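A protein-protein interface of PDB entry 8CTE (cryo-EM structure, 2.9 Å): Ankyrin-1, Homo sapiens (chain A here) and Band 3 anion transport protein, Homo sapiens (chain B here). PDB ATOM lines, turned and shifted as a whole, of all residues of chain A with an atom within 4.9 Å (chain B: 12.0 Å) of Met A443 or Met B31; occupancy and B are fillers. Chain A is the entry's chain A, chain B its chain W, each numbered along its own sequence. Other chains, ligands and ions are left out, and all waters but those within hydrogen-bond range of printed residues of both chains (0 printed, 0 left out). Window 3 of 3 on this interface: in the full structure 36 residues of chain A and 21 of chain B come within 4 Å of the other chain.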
ATOM      1  N   PHE A 372     -28.078  13.056 -15.991  1.00  0.00           N
ATOM      2  CA  PHE A 372     -27.047  13.702 -16.787  1.00  0.00           C
ATOM      3  C   PHE A 372     -27.507  13.891 -18.227  1.00  0.00           C
ATOM      4  O   PHE A 372     -27.972  12.952 -18.879  1.00  0.00           O
ATOM      5  CB  PHE A 372     -25.759  12.882 -16.755  1.00  0.00           C
ATOM      6  CG  PHE A 372     -24.918  13.123 -15.537  1.00  0.00           C
ATOM      7  CD1 PHE A 372     -25.267  12.573 -14.315  1.00  0.00           C
ATOM      8  CD2 PHE A 372     -23.772  13.896 -15.613  1.00  0.00           C
ATOM      9  CE1 PHE A 372     -24.493  12.794 -13.192  1.00  0.00           C
ATOM     10  CE2 PHE A 372     -22.993  14.121 -14.494  1.00  0.00           C
ATOM     11  CZ  PHE A 372     -23.354  13.568 -13.283  1.00  0.00           C
ATOM     12  N   LYS A 380     -18.010  17.241 -18.632  1.00  0.00           N
ATOM     13  CA  LYS A 380     -17.221  16.409 -17.728  1.00  0.00           C
ATOM     14  C   LYS A 380     -15.933  15.933 -18.387  1.00  0.00           C
ATOM     15  O   LYS A 380     -14.879  15.888 -17.741  1.00  0.00           O
ATOM     16  CB  LYS A 380     -18.045  15.211 -17.258  1.00  0.00           C
ATOM     17  CG  LYS A 380     -17.340  14.364 -16.216  1.00  0.00           C
ATOM     18  CD  LYS A 380     -18.243  13.269 -15.683  1.00  0.00           C
ATOM     19  CE  LYS A 380     -17.543  12.479 -14.592  1.00  0.00           C
ATOM     20  NZ  LYS A 380     -16.312  11.817 -15.101  1.00  0.00           N
ATOM     21  N   LEU A 405     -26.767  19.129 -10.279  1.00  0.00           N
ATOM     22  CA  LEU A 405     -25.496  19.521 -10.874  1.00  0.00           C
ATOM     23  C   LEU A 405     -25.723  20.191 -12.223  1.00  0.00           C
ATOM     24  O   LEU A 405     -26.261  19.575 -13.150  1.00  0.00           O
ATOM     25  CB  LEU A 405     -24.590  18.302 -11.031  1.00  0.00           C
ATOM     26  CG  LEU A 405     -24.030  17.674  -9.755  1.00  0.00           C
ATOM     27  CD1 LEU A 405     -23.479  16.291 -10.046  1.00  0.00           C
ATOM     28  CD2 LEU A 405     -22.953  18.561  -9.157  1.00  0.00           C
ATOM     29  N   HIS A 409     -21.165  23.325 -12.690  1.00  0.00           N
ATOM     30  CA  HIS A 409     -20.723  22.548 -11.532  1.00  0.00           C
ATOM     31  C   HIS A 409     -19.730  21.468 -11.938  1.00  0.00           C
ATOM     32  O   HIS A 409     -18.646  21.357 -11.351  1.00  0.00           O
ATOM     33  CB  HIS A 409     -21.925  21.905 -10.838  1.00  0.00           C
ATOM     34  CG  HIS A 409     -22.583  22.773  -9.814  1.00  0.00           C
ATOM     35  ND1 HIS A 409     -23.928  23.069  -9.846  1.00  0.00           N
ATOM     36  CD2 HIS A 409     -22.090  23.387  -8.713  1.00  0.00           C
ATOM     37  CE1 HIS A 409     -24.232  23.840  -8.818  1.00  0.00           C
ATOM     38  NE2 HIS A 409     -23.134  24.046  -8.113  1.00  0.00           N
ATOM     39  N   VAL A 410     -20.087  20.666 -12.942  1.00  0.00           N
ATOM     40  CA  VAL A 410     -19.233  19.566 -13.375  1.00  0.00           C
ATOM     41  C   VAL A 410     -17.927  20.093 -13.955  1.00  0.00           C
ATOM     42  O   VAL A 410     -16.848  19.552 -13.683  1.00  0.00           O
ATOM     43  CB  VAL A 410     -19.987  18.683 -14.385  1.00  0.00           C
ATOM     44  CG1 VAL A 410     -19.177  17.452 -14.715  1.00  0.00           C
ATOM     45  CG2 VAL A 410     -21.350  18.298 -13.836  1.00  0.00           C
ATOM     46  N   SER A 412     -16.397  22.944 -13.297  1.00  0.00           N
ATOM     47  CA  SER A 412     -15.553  23.491 -12.241  1.00  0.00           C
ATOM     48  C   SER A 412     -14.956  22.386 -11.380  1.00  0.00           C
ATOM     49  O   SER A 412     -13.801  22.485 -10.953  1.00  0.00           O
ATOM     50  CB  SER A 412     -16.355  24.468 -11.383  1.00  0.00           C
ATOM     51  OG  SER A 412     -16.842  25.546 -12.162  1.00  0.00           O
ATOM     52  N   PHE A 413     -15.729  21.332 -11.104  1.00  0.00           N
ATOM     53  CA  PHE A 413     -15.201  20.234 -10.300  1.00  0.00           C
ATOM     54  C   PHE A 413     -14.109  19.475 -11.045  1.00  0.00           C
ATOM     55  O   PHE A 413     -13.110  19.064 -10.442  1.00  0.00           O
ATOM     56  CB  PHE A 413     -16.327  19.289  -9.889  1.00  0.00           C
ATOM     57  CG  PHE A 413     -15.861  18.113  -9.082  1.00  0.00           C
ATOM     58  CD1 PHE A 413     -15.372  18.288  -7.797  1.00  0.00           C
ATOM     59  CD2 PHE A 413     -15.908  16.832  -9.605  1.00  0.00           C
ATOM     60  CE1 PHE A 413     -14.938  17.208  -7.050  1.00  0.00           C
ATOM     61  CE2 PHE A 413     -15.478  15.747  -8.863  1.00  0.00           C
ATOM     62  CZ  PHE A 413     -14.993  15.937  -7.584  1.00  0.00           C
ATOM     63  N   MET A 414     -14.276  19.281 -12.352  1.00  0.00           N
ATOM     64  CA  MET A 414     -13.281  18.566 -13.142  1.00  0.00           C
ATOM     65  C   MET A 414     -12.073  19.421 -13.497  1.00  0.00           C
ATOM     66  O   MET A 414     -11.063  18.873 -13.952  1.00  0.00           O
ATOM     67  CB  MET A 414     -13.917  18.021 -14.422  1.00  0.00           C
ATOM     68  CG  MET A 414     -14.962  16.944 -14.185  1.00  0.00           C
ATOM     69  SD  MET A 414     -14.296  15.517 -13.305  1.00  0.00           S
ATOM     70  CE  MET A 414     -13.027  14.975 -14.448  1.00  0.00           C
ATOM     71  N   GLU A 438     -23.998  23.603  -2.429  1.00  0.00           N
ATOM     72  CA  GLU A 438     -22.662  23.972  -2.872  1.00  0.00           C
ATOM     73  C   GLU A 438     -22.699  24.637  -4.243  1.00  0.00           C
ATOM     74  O   GLU A 438     -23.435  24.218  -5.141  1.00  0.00           O
ATOM     75  CB  GLU A 438     -21.762  22.738  -2.918  1.00  0.00           C
ATOM     76  CG  GLU A 438     -21.629  22.021  -1.590  1.00  0.00           C
ATOM     77  CD  GLU A 438     -20.818  20.746  -1.698  1.00  0.00           C
ATOM     78  OE1 GLU A 438     -20.403  20.396  -2.823  1.00  0.00           O
ATOM     79  OE2 GLU A 438     -20.594  20.093  -0.658  1.00  0.00           O
ATOM     80  N   THR A 439     -21.891  25.674  -4.399  1.00  0.00           N
ATOM     81  CA  THR A 439     -21.778  26.417  -5.646  1.00  0.00           C
ATOM     82  C   THR A 439     -20.641  25.852  -6.483  1.00  0.00           C
ATOM     83  O   THR A 439     -19.867  25.016  -6.012  1.00  0.00           O
ATOM     84  CB  THR A 439     -21.563  27.898  -5.332  1.00  0.00           C
ATOM     85  OG1 THR A 439     -20.377  28.056  -4.543  1.00  0.00           O
ATOM     86  CG2 THR A 439     -22.756  28.452  -4.565  1.00  0.00           C
ATOM     87  N   PRO A 440     -20.524  26.259  -7.757  1.00  0.00           N
ATOM     88  CA  PRO A 440     -19.331  25.857  -8.525  1.00  0.00           C
ATOM     89  C   PRO A 440     -18.027  26.320  -7.898  1.00  0.00           C
ATOM     90  O   PRO A 440     -16.990  25.672  -8.085  1.00  0.00           O
ATOM     91  CB  PRO A 440     -19.569  26.503  -9.896  1.00  0.00           C
ATOM     92  CG  PRO A 440     -21.042  26.558 -10.016  1.00  0.00           C
ATOM     93  CD  PRO A 440     -21.548  26.862  -8.633  1.00  0.00           C
ATOM     94  N   LEU A 441     -18.051  27.435  -7.162  1.00  0.00           N
ATOM     95  CA  LEU A 441     -16.867  27.854  -6.419  1.00  0.00           C
ATOM     96  C   LEU A 441     -16.515  26.843  -5.335  1.00  0.00           C
ATOM     97  O   LEU A 441     -15.332  26.586  -5.080  1.00  0.00           O
ATOM     98  CB  LEU A 441     -17.090  29.240  -5.814  1.00  0.00           C
ATOM     99  CG  LEU A 441     -15.905  29.853  -5.066  1.00  0.00           C
ATOM    100  CD1 LEU A 441     -14.698  29.968  -5.981  1.00  0.00           C
ATOM    101  CD2 LEU A 441     -16.281  31.208  -4.492  1.00  0.00           C
ATOM    102  N   HIS A 442     -17.527  26.267  -4.681  1.00  0.00           N
ATOM    103  CA  HIS A 442     -17.273  25.208  -3.707  1.00  0.00           C
ATOM    104  C   HIS A 442     -16.647  23.987  -4.369  1.00  0.00           C
ATOM    105  O   HIS A 442     -15.729  23.373  -3.814  1.00  0.00           O
ATOM    106  CB  HIS A 442     -18.568  24.819  -2.992  1.00  0.00           C
ATOM    107  CG  HIS A 442     -19.078  25.858  -2.043  1.00  0.00           C
ATOM    108  ND1 HIS A 442     -19.832  26.936  -2.453  1.00  0.00           N
ATOM    109  CD2 HIS A 442     -18.947  25.980  -0.701  1.00  0.00           C
ATOM    110  CE1 HIS A 442     -20.141  27.679  -1.407  1.00  0.00           C
ATOM    111  NE2 HIS A 442     -19.616  27.122  -0.330  1.00  0.00           N
ATOM    112  N   MET A 443     -17.141  23.615  -5.554  1.00  0.00           N
ATOM    113  CA  MET A 443     -16.580  22.476  -6.275  1.00  0.00           C
ATOM    114  C   MET A 443     -15.135  22.739  -6.683  1.00  0.00           C
ATOM    115  O   MET A 443     -14.282  21.848  -6.587  1.00  0.00           O
ATOM    116  CB  MET A 443     -17.436  22.167  -7.504  1.00  0.00           C
ATOM    117  CG  MET A 443     -18.930  22.100  -7.222  1.00  0.00           C
ATOM    118  SD  MET A 443     -19.451  20.575  -6.417  1.00  0.00           S
ATOM    119  CE  MET A 443     -19.397  19.429  -7.793  1.00  0.00           C
ATOM    120  N   ALA A 444     -14.842  23.958  -7.145  1.00  0.00           N
ATOM    121  CA  ALA A 444     -13.475  24.304  -7.519  1.00  0.00           C
ATOM    122  C   ALA A 444     -12.547  24.337  -6.311  1.00  0.00           C
ATOM    123  O   ALA A 444     -11.391  23.907  -6.408  1.00  0.00           O
ATOM    124  CB  ALA A 444     -13.454  25.652  -8.240  1.00  0.00           C
ATOM    125  N   ALA A 445     -13.026  24.843  -5.173  1.00  0.00           N
ATOM    126  CA  ALA A 445     -12.193  24.922  -3.979  1.00  0.00           C
ATOM    127  C   ALA A 445     -11.961  23.557  -3.345  1.00  0.00           C
ATOM    128  O   ALA A 445     -10.930  23.350  -2.696  1.00  0.00           O
ATOM    129  CB  ALA A 445     -12.824  25.872  -2.960  1.00  0.00           C
ATOM    130  N   ARG A 446     -12.896  22.623  -3.515  1.00  0.00           N
ATOM    131  CA  ARG A 446     -12.744  21.293  -2.941  1.00  0.00           C
ATOM    132  C   ARG A 446     -11.844  20.390  -3.773  1.00  0.00           C
ATOM    133  O   ARG A 446     -11.493  19.299  -3.311  1.00  0.00           O
ATOM    134  CB  ARG A 446     -14.115  20.633  -2.767  1.00  0.00           C
ATOM    135  CG  ARG A 446     -14.211  19.738  -1.543  1.00  0.00           C
ATOM    136  CD  ARG A 446     -15.575  19.073  -1.434  1.00  0.00           C
ATOM    137  NE  ARG A 446     -15.674  17.877  -2.261  1.00  0.00           N
ATOM    138  CZ  ARG A 446     -16.222  17.839  -3.469  1.00  0.00           C
ATOM    139  NH1 ARG A 446     -16.736  18.921  -4.030  1.00  0.00           N
ATOM    140  NH2 ARG A 446     -16.260  16.683  -4.127  1.00  0.00           N
ATOM    141  N   ALA A 447     -11.464  20.814  -4.978  1.00  0.00           N
ATOM    142  CA  ALA A 447     -10.582  20.038  -5.836  1.00  0.00           C
ATOM    143  C   ALA A 447      -9.270  20.747  -6.140  1.00  0.00           C
ATOM    144  O   ALA A 447      -8.460  20.213  -6.908  1.00  0.00           O
ATOM    145  CB  ALA A 447     -11.292  19.682  -7.148  1.00  0.00           C
ATOM    146  N   ILE B  26     -20.520  -0.710 -19.570  1.00  0.00           N
ATOM    147  CA  ILE B  26     -21.311   0.501 -19.763  1.00  0.00           C
ATOM    148  C   ILE B  26     -20.571   1.649 -19.085  1.00  0.00           C
ATOM    149  O   ILE B  26     -20.522   1.699 -17.849  1.00  0.00           O
ATOM    150  CB  ILE B  26     -22.732   0.352 -19.196  1.00  0.00           C
ATOM    151  N   PRO B  27     -19.977   2.578 -19.838  1.00  0.00           N
ATOM    152  CA  PRO B  27     -19.230   3.674 -19.203  1.00  0.00           C
ATOM    153  C   PRO B  27     -20.138   4.654 -18.478  1.00  0.00           C
ATOM    154  O   PRO B  27     -20.885   5.408 -19.112  1.00  0.00           O
ATOM    155  CB  PRO B  27     -18.513   4.343 -20.384  1.00  0.00           C
ATOM    156  CG  PRO B  27     -18.553   3.333 -21.497  1.00  0.00           C
ATOM    157  CD  PRO B  27     -19.830   2.584 -21.302  1.00  0.00           C
ATOM    158  N   GLU B  28     -20.080   4.653 -17.146  1.00  0.00           N
ATOM    159  CA  GLU B  28     -20.868   5.571 -16.329  1.00  0.00           C
ATOM    160  C   GLU B  28     -20.008   6.694 -15.760  1.00  0.00           C
ATOM    161  O   GLU B  28     -20.292   7.872 -15.997  1.00  0.00           O
ATOM    162  CB  GLU B  28     -21.566   4.803 -15.198  1.00  0.00           C
ATOM    163  N   SER B  29     -18.948   6.341 -15.025  1.00  0.00           N
ATOM    164  CA  SER B  29     -17.973   7.292 -14.487  1.00  0.00           C
ATOM    165  C   SER B  29     -18.662   8.370 -13.642  1.00  0.00           C
ATOM    166  O   SER B  29     -18.705   9.551 -13.994  1.00  0.00           O
ATOM    167  CB  SER B  29     -17.140   7.917 -15.613  1.00  0.00           C
ATOM    168  N   GLN B  30     -19.240   7.913 -12.532  1.00  0.00           N
ATOM    169  CA  GLN B  30     -19.943   8.810 -11.622  1.00  0.00           C
ATOM    170  C   GLN B  30     -19.005   9.888 -11.093  1.00  0.00           C
ATOM    171  O   GLN B  30     -17.887   9.600 -10.657  1.00  0.00           O
ATOM    172  CB  GLN B  30     -20.545   8.016 -10.463  1.00  0.00           C
ATOM    173  N   MET B  31     -19.471  11.140 -11.132  1.00  0.00           N
ATOM    174  CA  MET B  31     -18.632  12.270 -10.749  1.00  0.00           C
ATOM    175  C   MET B  31     -18.454  12.381  -9.240  1.00  0.00           C
ATOM    176  O   MET B  31     -17.532  13.069  -8.788  1.00  0.00           O
ATOM    177  CB  MET B  31     -19.225  13.568 -11.298  1.00  0.00           C
ATOM    178  CG  MET B  31     -18.235  14.719 -11.400  1.00  0.00           C
ATOM    179  SD  MET B  31     -19.039  16.327 -11.291  1.00  0.00           S
ATOM    180  CE  MET B  31     -19.767  16.222  -9.659  1.00  0.00           C
ATOM    181  N   GLU B  32     -19.309  11.727  -8.455  1.00  0.00           N
ATOM    182  CA  GLU B  32     -19.226  11.827  -7.003  1.00  0.00           C
ATOM    183  C   GLU B  32     -17.926  11.219  -6.493  1.00  0.00           C
ATOM    184  O   GLU B  32     -17.521  10.134  -6.921  1.00  0.00           O
ATOM    185  CB  GLU B  32     -20.425  11.132  -6.359  1.00  0.00           C
ATOM    186  N   GLU B  33     -17.271  11.926  -5.577  1.00  0.00           N
ATOM    187  CA  GLU B  33     -16.006  11.472  -5.016  1.00  0.00           C
ATOM    188  C   GLU B  33     -16.233  10.436  -3.920  1.00  0.00           C
ATOM    189  O   GLU B  33     -17.358  10.246  -3.457  1.00  0.00           O
ATOM    190  CB  GLU B  33     -15.208  12.655  -4.466  1.00  0.00           C
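The backbone carbonyl oxygen (O) of Ser B29 lies close to the side-chain amino group (NZ) of Lys A380 (3.5 Å).
Of the 8 printed residues of chain B, 2 touch a printed residue of chain A. Printed residues of chain B that touch a printed residue of chain A: Ser B29 and Met B31. Hydrophobic or aromatic side chains of chain B within 4 Å of the printed part of chain A: Met B31. Of the 18 printed residues of chain A, 5 touch a printed residue of chain B. Among the printed residues, 6 pairs touch across the chains. Among the printed residues, no Asp or Glu carboxylate lies within 4 Å of a Lys or Arg side-chain nitrogen of the other chain.
CE of Lys A380 touches CB of Met B31, 3.9 Å away. Met B31 touches Leu A405 (CE to CD1, 3.7 Å). Met B31 touches Val A410. Met B31 touches Phe A413 (O to CE2, 3.4 Å). CE of Met A443 touches CE of Met B31 (3.7 Å).
Printed residues of chain B within 4 Å of Leu A405: Met B31 (3.7 Å). His A409 touches none of the printed residues of chain B. Val A410 touches just one residue of chain B: Met B31. No residue of chain B comes within 4 Å of Ser A412. No residue of chain B comes within 4 Å of Glu A438. No residue of chain B comes within 4 Å of Pro A440. Leu A441 touches none of the printed residues of chain B. Met A443 touches one residue of chain B. No residue of chain B comes within 4 Å of Ala A444. No residue of chain B comes within 4 Å of Arg A446. Pro B27 touches none of the printed residues of chain A. Of the printed residues of chain A, Ser B29 touches Lys A380 (3.2 Å). Met B31 touches just these residues of chain A: Lys A380, Leu A405, Val A410, Phe A413 and Met A443.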
